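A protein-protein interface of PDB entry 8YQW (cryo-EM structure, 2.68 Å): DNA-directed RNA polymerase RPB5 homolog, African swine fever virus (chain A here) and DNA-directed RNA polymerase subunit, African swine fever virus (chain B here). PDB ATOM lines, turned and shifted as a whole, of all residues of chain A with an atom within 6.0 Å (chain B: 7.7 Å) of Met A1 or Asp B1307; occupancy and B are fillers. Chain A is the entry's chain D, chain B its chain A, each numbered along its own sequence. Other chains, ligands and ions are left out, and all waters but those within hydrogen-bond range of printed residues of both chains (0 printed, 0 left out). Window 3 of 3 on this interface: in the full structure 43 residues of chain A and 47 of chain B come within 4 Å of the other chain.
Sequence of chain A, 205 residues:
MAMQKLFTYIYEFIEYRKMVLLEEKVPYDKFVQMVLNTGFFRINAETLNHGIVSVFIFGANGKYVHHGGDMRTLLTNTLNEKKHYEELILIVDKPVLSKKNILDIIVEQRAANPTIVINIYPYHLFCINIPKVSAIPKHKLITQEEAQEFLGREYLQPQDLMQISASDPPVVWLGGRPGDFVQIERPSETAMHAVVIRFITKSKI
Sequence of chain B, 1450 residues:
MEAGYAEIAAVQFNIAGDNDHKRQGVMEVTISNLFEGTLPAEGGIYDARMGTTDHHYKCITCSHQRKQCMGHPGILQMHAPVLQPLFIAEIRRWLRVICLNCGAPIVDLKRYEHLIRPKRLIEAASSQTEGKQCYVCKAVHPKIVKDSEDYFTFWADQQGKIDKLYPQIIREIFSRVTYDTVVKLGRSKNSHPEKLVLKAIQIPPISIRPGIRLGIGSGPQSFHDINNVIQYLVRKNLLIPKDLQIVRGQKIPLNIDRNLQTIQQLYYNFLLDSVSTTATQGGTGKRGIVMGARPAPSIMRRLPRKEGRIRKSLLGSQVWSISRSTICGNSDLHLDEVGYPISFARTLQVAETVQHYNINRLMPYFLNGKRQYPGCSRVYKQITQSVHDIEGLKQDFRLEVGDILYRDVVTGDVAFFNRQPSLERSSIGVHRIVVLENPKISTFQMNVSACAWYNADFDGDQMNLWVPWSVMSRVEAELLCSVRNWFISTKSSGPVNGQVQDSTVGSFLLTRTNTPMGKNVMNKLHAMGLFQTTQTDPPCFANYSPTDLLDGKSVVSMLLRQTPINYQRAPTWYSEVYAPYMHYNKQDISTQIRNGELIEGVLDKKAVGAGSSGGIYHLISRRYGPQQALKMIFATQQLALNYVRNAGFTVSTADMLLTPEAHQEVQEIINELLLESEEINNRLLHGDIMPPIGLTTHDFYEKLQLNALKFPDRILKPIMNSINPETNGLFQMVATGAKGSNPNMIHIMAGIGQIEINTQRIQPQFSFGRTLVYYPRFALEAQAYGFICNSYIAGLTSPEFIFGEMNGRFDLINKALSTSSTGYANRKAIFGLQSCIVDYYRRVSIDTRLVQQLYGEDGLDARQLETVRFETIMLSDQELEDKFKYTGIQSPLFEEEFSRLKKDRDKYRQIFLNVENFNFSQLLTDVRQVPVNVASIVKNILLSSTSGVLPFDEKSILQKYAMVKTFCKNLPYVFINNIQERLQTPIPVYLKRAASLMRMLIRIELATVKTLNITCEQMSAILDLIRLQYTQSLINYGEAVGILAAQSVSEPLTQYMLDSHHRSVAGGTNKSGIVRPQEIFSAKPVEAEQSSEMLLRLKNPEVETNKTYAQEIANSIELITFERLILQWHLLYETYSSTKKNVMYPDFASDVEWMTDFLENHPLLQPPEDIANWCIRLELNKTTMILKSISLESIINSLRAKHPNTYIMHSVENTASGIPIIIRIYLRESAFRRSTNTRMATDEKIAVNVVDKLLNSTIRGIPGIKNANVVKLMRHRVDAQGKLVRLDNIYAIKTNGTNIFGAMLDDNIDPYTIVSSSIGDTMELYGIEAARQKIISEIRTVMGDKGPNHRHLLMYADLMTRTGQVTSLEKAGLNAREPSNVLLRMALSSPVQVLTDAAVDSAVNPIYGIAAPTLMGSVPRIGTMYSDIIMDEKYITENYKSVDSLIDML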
ATOM      1  N   MET A   1      -5.028   5.502  -9.745  1.00  0.00           N
ATOM      2  CA  MET A   1      -6.282   5.454 -10.488  1.00  0.00           C
ATOM      3  C   MET A   1      -6.628   6.814 -11.093  1.00  0.00           C
ATOM      4  O   MET A   1      -7.711   7.354 -10.881  1.00  0.00           O
ATOM      5  CB  MET A   1      -7.412   4.943  -9.584  1.00  0.00           C
ATOM      6  CG  MET A   1      -7.718   5.799  -8.362  1.00  0.00           C
ATOM      7  SD  MET A   1      -8.875   4.997  -7.236  1.00  0.00           S
ATOM      8  CE  MET A   1      -7.878   3.634  -6.641  1.00  0.00           C
ATOM      9  N   ALA A   2      -5.695   7.351 -11.882  1.00  0.00           N
ATOM     10  CA  ALA A   2      -5.886   8.675 -12.463  1.00  0.00           C
ATOM     11  C   ALA A   2      -7.040   8.705 -13.456  1.00  0.00           C
ATOM     12  O   ALA A   2      -7.724   9.725 -13.571  1.00  0.00           O
ATOM     13  CB  ALA A   2      -4.597   9.142 -13.136  1.00  0.00           C
ATOM     14  N   MET A   3      -7.271   7.608 -14.179  1.00  0.00           N
ATOM     15  CA  MET A   3      -8.324   7.601 -15.190  1.00  0.00           C
ATOM     16  C   MET A   3      -9.707   7.728 -14.563  1.00  0.00           C
ATOM     17  O   MET A   3     -10.563   8.455 -15.081  1.00  0.00           O
ATOM     18  CB  MET A   3      -8.229   6.330 -16.031  1.00  0.00           C
ATOM     19  CG  MET A   3      -6.965   6.246 -16.862  1.00  0.00           C
ATOM     20  SD  MET A   3      -6.858   7.559 -18.092  1.00  0.00           S
ATOM     21  CE  MET A   3      -5.758   6.806 -19.285  1.00  0.00           C
ATOM     22  N   GLN A   4      -9.947   7.027 -13.452  1.00  0.00           N
ATOM     23  CA  GLN A   4     -11.249   7.102 -12.799  1.00  0.00           C
ATOM     24  C   GLN A   4     -11.525   8.504 -12.275  1.00  0.00           C
ATOM     25  O   GLN A   4     -12.637   9.023 -12.426  1.00  0.00           O
ATOM     26  CB  GLN A   4     -11.328   6.079 -11.664  1.00  0.00           C
ATOM     27  CG  GLN A   4     -12.629   6.100 -10.861  1.00  0.00           C
ATOM     28  CD  GLN A   4     -13.876   5.919 -11.714  1.00  0.00           C
ATOM     29  OE1 GLN A   4     -14.334   6.847 -12.380  1.00  0.00           O
ATOM     30  NE2 GLN A   4     -14.435   4.714 -11.692  1.00  0.00           N
ATOM     31  N   LYS A   5     -10.524   9.135 -11.657  1.00  0.00           N
ATOM     32  CA  LYS A   5     -10.703  10.498 -11.171  1.00  0.00           C
ATOM     33  C   LYS A   5     -10.908  11.470 -12.323  1.00  0.00           C
ATOM     34  O   LYS A   5     -11.753  12.371 -12.241  1.00  0.00           O
ATOM     35  CB  LYS A   5      -9.501  10.911 -10.324  1.00  0.00           C
ATOM     36  CG  LYS A   5      -9.274  10.032  -9.111  1.00  0.00           C
ATOM     37  CD  LYS A   5     -10.476  10.028  -8.194  1.00  0.00           C
ATOM     38  CE  LYS A   5     -10.197   9.236  -6.933  1.00  0.00           C
ATOM     39  NZ  LYS A   5     -11.322   9.331  -5.967  1.00  0.00           N
ATOM     40  N   LEU A   6     -10.140  11.299 -13.403  1.00  0.00           N
ATOM     41  CA  LEU A   6     -10.279  12.165 -14.568  1.00  0.00           C
ATOM     42  C   LEU A   6     -11.677  12.071 -15.154  1.00  0.00           C
ATOM     43  O   LEU A   6     -12.299  13.091 -15.459  1.00  0.00           O
ATOM     44  CB  LEU A   6      -9.238  11.792 -15.623  1.00  0.00           C
ATOM     45  CG  LEU A   6      -7.838  12.390 -15.501  1.00  0.00           C
ATOM     46  CD1 LEU A   6      -6.865  11.588 -16.337  1.00  0.00           C
ATOM     47  CD2 LEU A   6      -7.842  13.838 -15.938  1.00  0.00           C
ATOM     48  N   CYS A 127      -7.850  15.572 -11.716  1.00  0.00           N
ATOM     49  CA  CYS A 127      -8.175  14.407 -10.909  1.00  0.00           C
ATOM     50  C   CYS A 127      -8.870  14.783  -9.608  1.00  0.00           C
ATOM     51  O   CYS A 127      -9.105  13.915  -8.764  1.00  0.00           O
ATOM     52  CB  CYS A 127      -6.912  13.597 -10.615  1.00  0.00           C
ATOM     53  SG  CYS A 127      -6.301  12.632 -12.013  1.00  0.00           S
ATOM     54  N   LEU B1098      -9.205  10.718   6.973  1.00  0.00           N
ATOM     55  CA  LEU B1098     -10.033   9.669   6.397  1.00  0.00           C
ATOM     56  C   LEU B1098     -11.305  10.255   5.797  1.00  0.00           C
ATOM     57  O   LEU B1098     -11.892  11.195   6.339  1.00  0.00           O
ATOM     58  CB  LEU B1098     -10.372   8.623   7.459  1.00  0.00           C
ATOM     59  CG  LEU B1098      -9.163   8.084   8.226  1.00  0.00           C
ATOM     60  CD1 LEU B1098      -9.575   7.050   9.251  1.00  0.00           C
ATOM     61  CD2 LEU B1098      -8.142   7.505   7.268  1.00  0.00           C
ATOM     62  N   LYS B1099     -11.724   9.691   4.662  1.00  0.00           N
ATOM     63  CA  LYS B1099     -12.881  10.219   3.945  1.00  0.00           C
ATOM     64  C   LYS B1099     -14.152  10.117   4.774  1.00  0.00           C
ATOM     65  O   LYS B1099     -15.096  10.886   4.563  1.00  0.00           O
ATOM     66  CB  LYS B1099     -13.051   9.475   2.621  1.00  0.00           C
ATOM     67  CG  LYS B1099     -14.170   9.998   1.736  1.00  0.00           C
ATOM     68  CD  LYS B1099     -14.297   9.173   0.470  1.00  0.00           C
ATOM     69  CE  LYS B1099     -13.157   9.453  -0.492  1.00  0.00           C
ATOM     70  NZ  LYS B1099     -13.234  10.828  -1.056  1.00  0.00           N
ATOM     71  N   ASN B1100     -14.191   9.189   5.725  1.00  0.00           N
ATOM     72  CA  ASN B1100     -15.389   8.951   6.512  1.00  0.00           C
ATOM     73  C   ASN B1100     -15.205   9.500   7.917  1.00  0.00           C
ATOM     74  O   ASN B1100     -14.307   9.039   8.638  1.00  0.00           O
ATOM     75  CB  ASN B1100     -15.699   7.459   6.560  1.00  0.00           C
ATOM     76  CG  ASN B1100     -17.126   7.179   6.955  1.00  0.00           C
ATOM     77  OD1 ASN B1100     -17.902   8.099   7.201  1.00  0.00           O
ATOM     78  ND2 ASN B1100     -17.483   5.903   7.017  1.00  0.00           N
ATOM     79  N   ILE B1113      -5.780   1.304   7.412  1.00  0.00           N
ATOM     80  CA  ILE B1113      -5.584   2.193   6.270  1.00  0.00           C
ATOM     81  C   ILE B1113      -4.157   2.727   6.251  1.00  0.00           C
ATOM     82  O   ILE B1113      -3.550   2.874   5.185  1.00  0.00           O
ATOM     83  CB  ILE B1113      -6.620   3.331   6.288  1.00  0.00           C
ATOM     84  CG1 ILE B1113      -8.031   2.771   6.127  1.00  0.00           C
ATOM     85  CG2 ILE B1113      -6.353   4.314   5.173  1.00  0.00           C
ATOM     86  CD1 ILE B1113      -9.113   3.749   6.503  1.00  0.00           C
ATOM     87  N   PHE B1301      -0.539  13.643  -5.023  1.00  0.00           N
ATOM     88  CA  PHE B1301      -1.310  13.008  -6.086  1.00  0.00           C
ATOM     89  C   PHE B1301      -1.568  11.537  -5.785  1.00  0.00           C
ATOM     90  O   PHE B1301      -2.642  11.012  -6.101  1.00  0.00           O
ATOM     91  CB  PHE B1301      -0.589  13.169  -7.421  1.00  0.00           C
ATOM     92  CG  PHE B1301      -1.424  12.793  -8.609  1.00  0.00           C
ATOM     93  CD1 PHE B1301      -2.782  13.052  -8.627  1.00  0.00           C
ATOM     94  CD2 PHE B1301      -0.850  12.191  -9.713  1.00  0.00           C
ATOM     95  CE1 PHE B1301      -3.548  12.710  -9.718  1.00  0.00           C
ATOM     96  CE2 PHE B1301      -1.611  11.849 -10.805  1.00  0.00           C
ATOM     97  CZ  PHE B1301      -2.962  12.110 -10.809  1.00  0.00           C
ATOM     98  N   GLY B1302      -0.594  10.852  -5.185  1.00  0.00           N
ATOM     99  CA  GLY B1302      -0.813   9.470  -4.794  1.00  0.00           C
ATOM    100  C   GLY B1302      -1.885   9.327  -3.732  1.00  0.00           C
ATOM    101  O   GLY B1302      -2.706   8.408  -3.785  1.00  0.00           O
ATOM    102  N   ALA B1303      -1.888  10.226  -2.746  1.00  0.00           N
ATOM    103  CA  ALA B1303      -2.938  10.211  -1.735  1.00  0.00           C
ATOM    104  C   ALA B1303      -4.249  10.757  -2.282  1.00  0.00           C
ATOM    105  O   ALA B1303      -5.323  10.402  -1.788  1.00  0.00           O
ATOM    106  CB  ALA B1303      -2.500  11.012  -0.511  1.00  0.00           C
ATOM    107  N   MET B1304      -4.179  11.621  -3.295  1.00  0.00           N
ATOM    108  CA  MET B1304      -5.388  12.144  -3.917  1.00  0.00           C
ATOM    109  C   MET B1304      -6.144  11.059  -4.672  1.00  0.00           C
ATOM    110  O   MET B1304      -7.361  11.166  -4.855  1.00  0.00           O
ATOM    111  CB  MET B1304      -5.024  13.292  -4.854  1.00  0.00           C
ATOM    112  CG  MET B1304      -6.192  14.040  -5.441  1.00  0.00           C
ATOM    113  SD  MET B1304      -5.615  15.440  -6.406  1.00  0.00           S
ATOM    114  CE  MET B1304      -4.965  16.474  -5.099  1.00  0.00           C
ATOM    115  N   LEU B1305      -5.444  10.016  -5.118  1.00  0.00           N
ATOM    116  CA  LEU B1305      -6.077   8.924  -5.843  1.00  0.00           C
ATOM    117  C   LEU B1305      -6.638   7.847  -4.926  1.00  0.00           C
ATOM    118  O   LEU B1305      -7.379   6.982  -5.400  1.00  0.00           O
ATOM    119  CB  LEU B1305      -5.079   8.297  -6.819  1.00  0.00           C
ATOM    120  CG  LEU B1305      -4.557   9.205  -7.936  1.00  0.00           C
ATOM    121  CD1 LEU B1305      -3.440   8.525  -8.704  1.00  0.00           C
ATOM    122  CD2 LEU B1305      -5.679   9.605  -8.869  1.00  0.00           C
ATOM    123  N   ASP B1306      -6.310   7.875  -3.639  1.00  0.00           N
ATOM    124  CA  ASP B1306      -6.828   6.890  -2.702  1.00  0.00           C
ATOM    125  C   ASP B1306      -8.283   7.184  -2.360  1.00  0.00           C
ATOM    126  O   ASP B1306      -8.699   8.341  -2.262  1.00  0.00           O
ATOM    127  CB  ASP B1306      -5.986   6.869  -1.426  1.00  0.00           C
ATOM    128  CG  ASP B1306      -6.109   5.562  -0.673  1.00  0.00           C
ATOM    129  OD1 ASP B1306      -6.709   4.614  -1.221  1.00  0.00           O
ATOM    130  OD2 ASP B1306      -5.610   5.480   0.469  1.00  0.00           O
ATOM    131  N   ASP B1307      -9.060   6.119  -2.179  1.00  0.00           N
ATOM    132  CA  ASP B1307     -10.463   6.249  -1.815  1.00  0.00           C
ATOM    133  C   ASP B1307     -10.697   6.226  -0.312  1.00  0.00           C
ATOM    134  O   ASP B1307     -11.827   6.469   0.125  1.00  0.00           O
ATOM    135  CB  ASP B1307     -11.286   5.139  -2.476  1.00  0.00           C
ATOM    136  CG  ASP B1307     -11.508   5.382  -3.955  1.00  0.00           C
ATOM    137  OD1 ASP B1307     -11.608   6.561  -4.355  1.00  0.00           O
ATOM    138  OD2 ASP B1307     -11.580   4.396  -4.718  1.00  0.00           O
ATOM    139  N   ASN B1308      -9.670   5.942   0.484  1.00  0.00           N
ATOM    140  CA  ASN B1308      -9.770   5.979   1.935  1.00  0.00           C
ATOM    141  C   ASN B1308      -9.309   7.306   2.520  1.00  0.00           C
ATOM    142  O   ASN B1308      -9.331   7.471   3.743  1.00  0.00           O
ATOM    143  CB  ASN B1308      -8.955   4.839   2.550  1.00  0.00           C
ATOM    144  CG  ASN B1308      -9.548   3.480   2.262  1.00  0.00           C
ATOM    145  OD1 ASN B1308     -10.748   3.265   2.423  1.00  0.00           O
ATOM    146  ND2 ASN B1308      -8.707   2.552   1.827  1.00  0.00           N
ATOM    147  N   ILE B1309      -8.898   8.248   1.679  1.00  0.00           N
ATOM    148  CA  ILE B1309      -8.390   9.542   2.111  1.00  0.00           C
ATOM    149  C   ILE B1309      -9.307  10.625   1.565  1.00  0.00           C
ATOM    150  O   ILE B1309      -9.758  10.547   0.418  1.00  0.00           O
ATOM    151  CB  ILE B1309      -6.938   9.759   1.637  1.00  0.00           C
ATOM    152  CG1 ILE B1309      -6.056   8.584   2.064  1.00  0.00           C
ATOM    153  CG2 ILE B1309      -6.377  11.066   2.170  1.00  0.00           C
ATOM    154  CD1 ILE B1309      -6.036   8.350   3.555  1.00  0.00           C
ATOM    155  N   ASP B1310      -9.600  11.619   2.391  1.00  0.00           N
ATOM    156  CA  ASP B1310     -10.336  12.782   1.913  1.00  0.00           C
ATOM    157  C   ASP B1310      -9.401  13.632   1.063  1.00  0.00           C
ATOM    158  O   ASP B1310      -8.411  14.158   1.589  1.00  0.00           O
ATOM    159  CB  ASP B1310     -10.879  13.590   3.086  1.00  0.00           C
ATOM    160  CG  ASP B1310     -11.973  14.553   2.675  1.00  0.00           C
ATOM    161  OD1 ASP B1310     -12.423  14.489   1.514  1.00  0.00           O
ATOM    162  OD2 ASP B1310     -12.382  15.380   3.514  1.00  0.00           O
ATOM    163  N   PRO B1311      -9.670  13.803  -0.234  1.00  0.00           N
ATOM    164  CA  PRO B1311      -8.693  14.474  -1.099  1.00  0.00           C
ATOM    165  C   PRO B1311      -8.667  15.982  -0.955  1.00  0.00           C
ATOM    166  O   PRO B1311      -7.688  16.606  -1.383  1.00  0.00           O
ATOM    167  CB  PRO B1311      -9.142  14.067  -2.506  1.00  0.00           C
ATOM    168  CG  PRO B1311     -10.604  13.863  -2.374  1.00  0.00           C
ATOM    169  CD  PRO B1311     -10.842  13.327  -0.989  1.00  0.00           C
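OD1 of Asp B1307 is in salt-bridge range of NZ of Lys A5. O of Leu B1305 lies close to SD of Met A1, at 3.1 Å. The side-chain carboxylate (OD2) of Asp B1307 lies close to the side-chain sulfur (SD) of Met A1 (3.7 Å).
The backbone carbonyl oxygen (O) of Ala A2 is in hydrogen-bond range of the side-chain sulfur (SG) of Cys A127.
Among the printed residues, pairs that only touch across the chains: Ala A2 with Leu B1305, Lys A5 with Leu B1305 and Cys A127 with Phe B1301.
Of chain B, only Leu B1305 (3.1 Å) and Asp B1307 (3.7 Å) come within 4 Å of Met A1. Asp B1307 touches two residues of chain A. Of the printed residues of chain A, Leu B1305 touches Met A1, Ala A2 and Lys A5. Printed residues of chain B within 4 Å of Lys A5: Leu B1305 and Asp B1307. Printed residues of chain B within 4 Å of Ala A2: Leu B1305 (3.7 Å). Printed residues of chain A within 4 Å of Phe B1301: Cys A127. Ile B1113 touches none of the printed residues of chain A. Leu B1098 touches none of the printed residues of chain A. The nearest residue of chain B that does not touch Met A1 is Asp B1306 (5.2 Å). The nearest printed residue of chain B that does not touch Ala A2 is Phe B1301 (4.1 Å).
Of the 15 printed residues of chain B, 3 touch a printed residue of chain A. Hydrophobic or aromatic side chains of chain B within 4 Å of the printed part of chain A: Phe B1301 and Leu B1305. Of the 7 printed residues of chain A, 4 touch a printed residue of chain B.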
